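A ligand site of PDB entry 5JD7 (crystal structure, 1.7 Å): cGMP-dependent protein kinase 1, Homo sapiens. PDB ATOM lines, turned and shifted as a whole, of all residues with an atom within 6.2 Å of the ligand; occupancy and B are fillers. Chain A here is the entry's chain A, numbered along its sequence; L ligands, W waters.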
ATOM      1  N   ILE A  48      10.997  12.137 -13.462  1.00  0.00           N
ATOM      2  CA  ILE A  48      10.618  13.361 -12.796  1.00  0.00           C
ATOM      3  C   ILE A  48       9.855  12.990 -11.544  1.00  0.00           C
ATOM      4  O   ILE A  48       9.062  12.042 -11.551  1.00  0.00           O
ATOM      5  CB  ILE A  48       9.719  14.257 -13.678  1.00  0.00           C
ATOM      6  CG1 ILE A  48      10.503  14.839 -14.851  1.00  0.00           C
ATOM      7  CG2 ILE A  48       9.048  15.353 -12.805  1.00  0.00           C
ATOM      8  CD1 ILE A  48       9.604  15.633 -15.821  1.00  0.00           C
ATOM      9  N   THR A  56      14.017  21.405 -17.343  1.00  0.00           N
ATOM     10  CA  THR A  56      14.271  20.570 -18.519  1.00  0.00           C
ATOM     11  C   THR A  56      12.984  20.034 -19.099  1.00  0.00           C
ATOM     12  O   THR A  56      12.020  19.729 -18.383  1.00  0.00           O
ATOM     13  CB  THR A  56      15.183  19.390 -18.184  1.00  0.00           C
ATOM     14  OG1 THR A  56      14.795  18.804 -16.934  1.00  0.00           O
ATOM     15  CG2 THR A  56      16.609  19.862 -18.158  1.00  0.00           C
ATOM     16  N   VAL A  67       2.687   8.570 -16.222  1.00  0.00           N
ATOM     17  CA  VAL A  67       2.531   9.839 -15.516  1.00  0.00           C
ATOM     18  C   VAL A  67       1.561   9.624 -14.377  1.00  0.00           C
ATOM     19  O   VAL A  67       0.481   9.055 -14.564  1.00  0.00           O
ATOM     20  CB  VAL A  67       2.032  10.978 -16.420  1.00  0.00           C
ATOM     21  CG1 VAL A  67       2.058  12.308 -15.648  1.00  0.00           C
ATOM     22  CG2 VAL A  67       2.862  11.082 -17.673  1.00  0.00           C
ATOM     23  N   ARG A  69       0.156  11.507 -10.402  1.00  0.00           N
ATOM     24  CA  ARG A  69       0.150  12.710  -9.590  1.00  0.00           C
ATOM     25  C   ARG A  69      -0.568  12.454  -8.268  1.00  0.00           C
ATOM     26  O   ARG A  69      -1.625  11.813  -8.256  1.00  0.00           O
ATOM     27  CB  ARG A  69      -0.530  13.859 -10.334  1.00  0.00           C
ATOM     28  CG  ARG A  69      -0.627  15.146  -9.545  1.00  0.00           C
ATOM     29  CD  ARG A  69      -1.219  16.292 -10.352  1.00  0.00           C
ATOM     30  NE  ARG A  69      -1.955  17.165  -9.457  1.00  0.00           N
ATOM     31  CZ  ARG A  69      -1.387  18.039  -8.635  1.00  0.00           C
ATOM     32  NH1 ARG A  69      -0.064  18.179  -8.603  1.00  0.00           N
ATOM     33  NH2 ARG A  69      -2.139  18.780  -7.856  1.00  0.00           N
ATOM     34  N   LEU A  80      -2.230   8.962 -14.288  1.00  0.00           N
ATOM     35  CA  LEU A  80      -2.763   9.930 -15.242  1.00  0.00           C
ATOM     36  C   LEU A  80      -2.735   9.389 -16.661  1.00  0.00           C
ATOM     37  O   LEU A  80      -3.783   9.252 -17.304  1.00  0.00           O
ATOM     38  CB  LEU A  80      -1.993  11.245 -15.157  1.00  0.00           C
ATOM     39  CG  LEU A  80      -1.913  11.975 -13.814  1.00  0.00           C
ATOM     40  CD1 LEU A  80      -1.506  13.448 -14.001  1.00  0.00           C
ATOM     41  CD2 LEU A  80      -3.234  11.850 -13.072  1.00  0.00           C
ATOM     42  N   ARG A  81      -1.555   9.056 -17.172  1.00  0.00           N
ATOM     43  CA  ARG A  81      -1.477   8.600 -18.552  1.00  0.00           C
ATOM     44  C   ARG A  81      -0.107   7.995 -18.821  1.00  0.00           C
ATOM     45  O   ARG A  81       0.834   8.124 -18.034  1.00  0.00           O
ATOM     46  CB  ARG A  81      -1.757   9.733 -19.535  1.00  0.00           C
ATOM     47  CG  ARG A  81      -0.587  10.722 -19.665  1.00  0.00           C
ATOM     48  CD  ARG A  81      -1.008  11.950 -20.427  1.00  0.00           C
ATOM     49  NE  ARG A  81      -1.823  12.819 -19.578  1.00  0.00           N
ATOM     50  CZ  ARG A  81      -3.115  13.072 -19.762  1.00  0.00           C
ATOM     51  NH1 ARG A  81      -3.789  12.530 -20.774  1.00  0.00           N
ATOM     52  NH2 ARG A  81      -3.728  13.882 -18.918  1.00  0.00           N
ATOM     53  N   LEU A  83       2.783   7.806 -21.922  1.00  0.00           N
ATOM     54  CA  LEU A  83       3.261   8.506 -23.114  1.00  0.00           C
ATOM     55  C   LEU A  83       4.328   7.654 -23.781  1.00  0.00           C
ATOM     56  O   LEU A  83       5.016   6.864 -23.130  1.00  0.00           O
ATOM     57  CB  LEU A  83       3.821   9.916 -22.777  1.00  0.00           C
ATOM     58  CG  LEU A  83       2.944  10.939 -22.055  1.00  0.00           C
ATOM     59  CD1 LEU A  83       3.784  12.143 -21.607  1.00  0.00           C
ATOM     60  CD2 LEU A  83       1.837  11.431 -22.944  1.00  0.00           C
ATOM     61  N   TRP A  88       5.976  14.090 -25.275  1.00  0.00           N
ATOM     62  CA  TRP A  88       6.913  14.961 -24.574  1.00  0.00           C
ATOM     63  C   TRP A  88       6.272  15.377 -23.259  1.00  0.00           C
ATOM     64  O   TRP A  88       5.061  15.254 -23.071  1.00  0.00           O
ATOM     65  CB  TRP A  88       7.273  16.196 -25.404  1.00  0.00           C
ATOM     66  CG  TRP A  88       6.113  16.823 -26.087  1.00  0.00           C
ATOM     67  CD1 TRP A  88       5.717  16.627 -27.374  1.00  0.00           C
ATOM     68  CD2 TRP A  88       5.152  17.735 -25.511  1.00  0.00           C
ATOM     69  NE1 TRP A  88       4.575  17.354 -27.649  1.00  0.00           N
ATOM     70  CE2 TRP A  88       4.217  18.051 -26.531  1.00  0.00           C
ATOM     71  CE3 TRP A  88       5.011  18.319 -24.255  1.00  0.00           C
ATOM     72  CZ2 TRP A  88       3.152  18.912 -26.323  1.00  0.00           C
ATOM     73  CZ3 TRP A  88       3.954  19.168 -24.044  1.00  0.00           C
ATOM     74  CH2 TRP A  88       3.029  19.462 -25.083  1.00  0.00           C
ATOM     75  N   PHE A  89       7.092  15.890 -22.358  1.00  0.00           N
ATOM     76  CA  PHE A  89       6.616  16.261 -21.038  1.00  0.00           C
ATOM     77  C   PHE A  89       7.676  17.118 -20.353  1.00  0.00           C
ATOM     78  O   PHE A  89       8.815  17.250 -20.823  1.00  0.00           O
ATOM     79  CB  PHE A  89       6.304  15.015 -20.200  1.00  0.00           C
ATOM     80  CG  PHE A  89       7.501  14.089 -20.034  1.00  0.00           C
ATOM     81  CD1 PHE A  89       7.712  13.045 -20.893  1.00  0.00           C
ATOM     82  CD2 PHE A  89       8.429  14.298 -19.017  1.00  0.00           C
ATOM     83  CE1 PHE A  89       8.791  12.219 -20.762  1.00  0.00           C
ATOM     84  CE2 PHE A  89       9.505  13.507 -18.868  1.00  0.00           C
ATOM     85  CZ  PHE A  89       9.704  12.445 -19.738  1.00  0.00           C
ATOM     86  N   GLY A  90       7.278  17.724 -19.242  1.00  0.00           N
ATOM     87  CA  GLY A  90       8.144  18.564 -18.454  1.00  0.00           C
ATOM     88  C   GLY A  90       7.972  20.048 -18.739  1.00  0.00           C
ATOM     89  O   GLY A  90       8.786  20.852 -18.272  1.00  0.00           O
ATOM     90  N   GLU A  91       6.957  20.427 -19.507  1.00  0.00           N
ATOM     91  CA  GLU A  91       6.804  21.831 -19.874  1.00  0.00           C
ATOM     92  C   GLU A  91       6.241  22.679 -18.734  1.00  0.00           C
ATOM     93  O   GLU A  91       6.447  23.899 -18.697  1.00  0.00           O
ATOM     94  CB  GLU A  91       5.919  21.981 -21.126  1.00  0.00           C
ATOM     95  CG  GLU A  91       4.398  21.963 -20.930  1.00  0.00           C
ATOM     96  CD  GLU A  91       3.817  20.594 -20.588  1.00  0.00           C
ATOM     97  OE1 GLU A  91       4.565  19.577 -20.624  1.00  0.00           O
ATOM     98  OE2 GLU A  91       2.595  20.537 -20.291  1.00  0.00           O
ATOM     99  N   LYS A  92       5.477  22.103 -17.798  1.00  0.00           N
ATOM    100  CA  LYS A  92       4.772  22.984 -16.870  1.00  0.00           C
ATOM    101  C   LYS A  92       5.773  23.727 -15.963  1.00  0.00           C
ATOM    102  O   LYS A  92       5.602  24.918 -15.685  1.00  0.00           O
ATOM    103  CB  LYS A  92       3.749  22.194 -16.048  1.00  0.00           C
ATOM    104  CG  LYS A  92       2.597  21.645 -16.918  1.00  0.00           C
ATOM    105  CD  LYS A  92       1.369  21.340 -16.059  1.00  0.00           C
ATOM    106  CE  LYS A  92       0.704  22.624 -15.594  1.00  0.00           C
ATOM    107  N   ALA A  93       6.828  23.046 -15.535  1.00  0.00           N
ATOM    108  CA  ALA A  93       7.884  23.688 -14.750  1.00  0.00           C
ATOM    109  C   ALA A  93       8.670  24.713 -15.540  1.00  0.00           C
ATOM    110  O   ALA A  93       9.469  25.456 -14.962  1.00  0.00           O
ATOM    111  CB  ALA A  93       8.839  22.653 -14.190  1.00  0.00           C
ATOM    112  N   LEU A  94       8.468  24.755 -16.855  1.00  0.00           N
ATOM    113  CA  LEU A  94       9.100  25.744 -17.710  1.00  0.00           C
ATOM    114  C   LEU A  94       8.132  26.866 -18.093  1.00  0.00           C
ATOM    115  O   LEU A  94       8.476  27.719 -18.917  1.00  0.00           O
ATOM    116  CB  LEU A  94       9.636  25.072 -18.969  1.00  0.00           C
ATOM    117  CG  LEU A  94      10.815  24.142 -18.735  1.00  0.00           C
ATOM    118  CD1 LEU A  94      11.020  23.124 -19.897  1.00  0.00           C
ATOM    119  CD2 LEU A  94      12.033  24.959 -18.539  1.00  0.00           C
ATOM    120  N   VAL A  99       8.052  24.330 -10.464  1.00  0.00           N
ATOM    121  CA  VAL A  99       7.783  23.105  -9.722  1.00  0.00           C
ATOM    122  C   VAL A  99       7.227  22.032 -10.661  1.00  0.00           C
ATOM    123  O   VAL A  99       6.433  22.312 -11.568  1.00  0.00           O
ATOM    124  CB  VAL A  99       6.816  23.377  -8.557  1.00  0.00           C
ATOM    125  CG1 VAL A  99       5.453  23.759  -9.095  1.00  0.00           C
ATOM    126  CG2 VAL A  99       6.725  22.129  -7.656  1.00  0.00           C
ATOM    127  N   ARG A 100       7.647  20.796 -10.433  1.00  0.00           N
ATOM    128  CA  ARG A 100       7.114  19.668 -11.179  1.00  0.00           C
ATOM    129  C   ARG A 100       5.764  19.301 -10.607  1.00  0.00           C
ATOM    130  O   ARG A 100       5.633  19.170  -9.396  1.00  0.00           O
ATOM    131  CB  ARG A 100       8.061  18.475 -11.090  1.00  0.00           C
ATOM    132  CG  ARG A 100       9.407  18.730 -11.668  1.00  0.00           C
ATOM    133  CD  ARG A 100       9.286  18.997 -13.173  1.00  0.00           C
ATOM    134  NE  ARG A 100      10.585  18.859 -13.836  1.00  0.00           N
ATOM    135  CZ  ARG A 100      10.836  19.157 -15.102  1.00  0.00           C
ATOM    136  NH1 ARG A 100       9.885  19.643 -15.932  1.00  0.00           N
ATOM    137  NH2 ARG A 100      12.088  18.996 -15.539  1.00  0.00           N
ATOM    138  N   THR A 101       4.755  19.136 -11.465  1.00  0.00           N
ATOM    139  CA  THR A 101       3.374  18.937 -11.040  1.00  0.00           C
ATOM    140  C   THR A 101       2.922  17.498 -11.134  1.00  0.00           C
ATOM    141  O   THR A 101       1.756  17.213 -10.850  1.00  0.00           O
ATOM    142  CB  THR A 101       2.449  19.834 -11.843  1.00  0.00           C
ATOM    143  OG1 THR A 101       2.370  19.387 -13.225  1.00  0.00           O
ATOM    144  CG2 THR A 101       2.926  21.242 -11.771  1.00  0.00           C
ATOM    145  N   ALA A 102       3.810  16.570 -11.501  1.00  0.00           N
ATOM    146  CA  ALA A 102       3.474  15.161 -11.611  1.00  0.00           C
ATOM    147  C   ALA A 102       4.750  14.346 -11.658  1.00  0.00           C
ATOM    148  O   ALA A 102       5.821  14.855 -11.994  1.00  0.00           O
ATOM    149  CB  ALA A 102       2.631  14.879 -12.859  1.00  0.00           C
ATOM    150  N   ASN A 103       4.629  13.065 -11.334  1.00  0.00           N
ATOM    151  CA  ASN A 103       5.724  12.120 -11.551  1.00  0.00           C
ATOM    152  C   ASN A 103       5.644  11.552 -12.960  1.00  0.00           C
ATOM    153  O   ASN A 103       4.560  11.308 -13.496  1.00  0.00           O
ATOM    154  CB  ASN A 103       5.677  10.938 -10.576  1.00  0.00           C
ATOM    155  CG  ASN A 103       5.522  11.365  -9.156  1.00  0.00           C
ATOM    156  OD1 ASN A 103       6.453  11.879  -8.532  1.00  0.00           O
ATOM    157  ND2 ASN A 103       4.318  11.159  -8.622  1.00  0.00           N
ATOM    158  N   VAL A 104       6.823  11.282 -13.525  1.00  0.00           N
ATOM    159  CA  VAL A 104       6.947  10.568 -14.799  1.00  0.00           C
ATOM    160  C   VAL A 104       7.929   9.425 -14.563  1.00  0.00           C
ATOM    161  O   VAL A 104       9.096   9.673 -14.209  1.00  0.00           O
ATOM    162  CB  VAL A 104       7.443  11.471 -15.940  1.00  0.00           C
ATOM    163  CG1 VAL A 104       7.366  10.715 -17.256  1.00  0.00           C
ATOM    164  CG2 VAL A 104       6.655  12.792 -16.009  1.00  0.00           C
ATOM    165  N   TYR A 135      -4.479  19.460 -19.597  1.00  0.00           N
ATOM    166  CA  TYR A 135      -4.642  18.057 -19.224  1.00  0.00           C
ATOM    167  C   TYR A 135      -6.043  17.686 -18.694  1.00  0.00           C
ATOM    168  O   TYR A 135      -6.318  17.816 -17.504  1.00  0.00           O
ATOM    169  CB  TYR A 135      -3.592  17.707 -18.207  1.00  0.00           C
ATOM    170  CG  TYR A 135      -2.201  17.821 -18.791  1.00  0.00           C
ATOM    171  CD1 TYR A 135      -1.425  18.957 -18.584  1.00  0.00           C
ATOM    172  CD2 TYR A 135      -1.681  16.806 -19.566  1.00  0.00           C
ATOM    173  CE1 TYR A 135      -0.146  19.054 -19.136  1.00  0.00           C
ATOM    174  CE2 TYR A 135      -0.416  16.888 -20.112  1.00  0.00           C
ATOM    175  CZ  TYR A 135       0.343  18.025 -19.891  1.00  0.00           C
ATOM    176  OH  TYR A 135       1.623  18.089 -20.444  1.00  0.00           O
HETATM  177  N1  LIG L   1      -1.043  16.690 -15.488  1.00  0.00           N
HETATM  178  C1  LIG L   1       5.006  16.265 -16.259  1.00  0.00           C
HETATM  179  C2  LIG L   1       1.619  14.449 -18.585  1.00  0.00           C
HETATM  180  C3  LIG L   1       0.075  15.268 -17.286  1.00  0.00           C
HETATM  181  C4  LIG L   1      -1.175  15.683 -16.495  1.00  0.00           C
HETATM  182  C5  LIG L   1      -1.940  17.272 -14.630  1.00  0.00           C
HETATM  183  C6  LIG L   1      -1.787  19.109 -12.770  1.00  0.00           C
HETATM  184  C7  LIG L   1      -0.941  20.228 -12.352  1.00  0.00           C
HETATM  185  P1  LIG L   1       5.938  19.071 -15.319  1.00  0.00           P
HETATM  186  O1  LIG L   1       4.160  15.350 -16.442  1.00  0.00           O
HETATM  187  O2  LIG L   1       5.156  18.877 -16.803  1.00  0.00           O
HETATM  188  O3  LIG L   1       6.607  17.567 -14.911  1.00  0.00           O
HETATM  189  O4  LIG L   1       4.471  17.470 -19.085  1.00  0.00           O
HETATM  190  O5  LIG L   1       4.992  19.507 -14.263  1.00  0.00           O
HETATM  191  O6  LIG L   1       7.129  20.029 -15.495  1.00  0.00           O
HETATM  192  O7  LIG L   1      -2.260  15.181 -16.703  1.00  0.00           O
HETATM  193  N2  LIG L   1       2.204  15.385 -17.791  1.00  0.00           N
HETATM  194  N3  LIG L   1       0.307  14.369 -18.305  1.00  0.00           N
HETATM  195  N4  LIG L   1       1.329  16.888 -15.996  1.00  0.00           N
HETATM  196  N5  LIG L   1       0.084  18.211 -14.247  1.00  0.00           N
HETATM  197  C8  LIG L   1       4.253  17.731 -16.821  1.00  0.00           C
HETATM  198  C9  LIG L   1       3.622  17.357 -17.904  1.00  0.00           C
HETATM  199  C10 LIG L   1       3.371  15.744 -17.790  1.00  0.00           C
HETATM  200  C11 LIG L   1       5.581  16.420 -14.865  1.00  0.00           C
HETATM  201  C12 LIG L   1       1.241  15.864 -17.007  1.00  0.00           C
HETATM  202  C13 LIG L   1       0.178  17.287 -15.243  1.00  0.00           C
HETATM  203  C14 LIG L   1      -1.234  18.196 -13.875  1.00  0.00           C
HETATM  204  C15 LIG L   1      -3.153  18.861 -12.143  1.00  0.00           C
HETATM  205  C16 LIG L   1      -3.624  19.792 -11.057  1.00  0.00           C
HETATM  206  C17 LIG L   1      -1.426  21.159 -11.268  1.00  0.00           C
HETATM  207  C18 LIG L   1      -2.781  20.928 -10.630  1.00  0.00           C
HETATM  208  O   HOH W   1       2.741  15.706 -21.414  1.00  0.00           O
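O of Val 67 is in hydrogen-bond range of N of Leu 80 (2.7 Å). The guanidinium group of Arg 69 sits at hydrogen-bond distance from the backbone carbonyl oxygen of Thr 101, 3.0 Å away. The backbone carbonyl oxygen of Thr 56 is in hydrogen-bond range of the guanidinium group of Arg 100, at 2.9 Å. The side-chain hydroxyl (OH) of Tyr 135 lies within hydrogen-bond range of the side-chain carboxylate (OE2) of Glu 91 (2.6 Å). O of Arg 81 is in hydrogen-bond range of N of Val 67, at 2.6 Å. NH1 of Arg 100 sits at hydrogen-bond distance from O of Gly 90. N of Val 104 sits at hydrogen-bond distance from O of Ile 48.
Residues that only touch the ligand: Phe 89 (3.1 Å), Ala 102 (3.3 Å), Leu 80 (3.3 Å), Arg 69 (3.4 Å), Val 104 (3.6 Å), Val 67 (3.7 Å) and Ile 48 (3.7 Å). Hydrophobic or aromatic side chains within 4 Å of the ligand: Ile 48, Val 67, Leu 80, Phe 89, Ala 93, Ala 102, Val 104 and Tyr 135. 15 residues have an atom within 4 Å of the ligand: Ile 48, Val 67, Arg 69, Leu 80, Arg 81, Phe 89, Gly 90, Glu 91, Lys 92, Ala 93, Arg 100, Thr 101, Ala 102, Val 104 and Tyr 135. The nearest printed residue that does not touch the ligand is Val 99 (4.1 Å).
Water W1 lies within hydrogen-bond range of OH of Tyr 135, O of Trp 88 and O4 of the ligand.
An oxygen (O6) of the ligand lies within salt-bridge range of the guanidinium group of Arg 100, at 2.8 Å. An oxygen (O4) of the ligand sits at hydrogen-bond distance from the backbone NH of Gly 90 (2.8 Å). An oxygen (O5) of the ligand lies within hydrogen-bond range of the backbone NH (N) of Thr 101 (2.8 Å). An oxygen (O6) of the ligand sits at hydrogen-bond distance from the backbone NH (N) of Ala 93, 3.0 Å away. O4 of the ligand sits at hydrogen-bond distance from OH of Tyr 135 (3.2 Å). An oxygen (O2) of the ligand lies within hydrogen-bond range of the backbone NH (N) of Lys 92, at 3.4 Å. OE1 of Glu 91 sits at hydrogen-bond distance from O4 of the ligand. N3 of the ligand is in hydrogen-bond range of NE of Arg 81 (2.9 Å). The side-chain hydroxyl (OG1) of Thr 101 is in hydrogen-bond range of a nitrogen (N5) of the ligand (2.8 Å).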
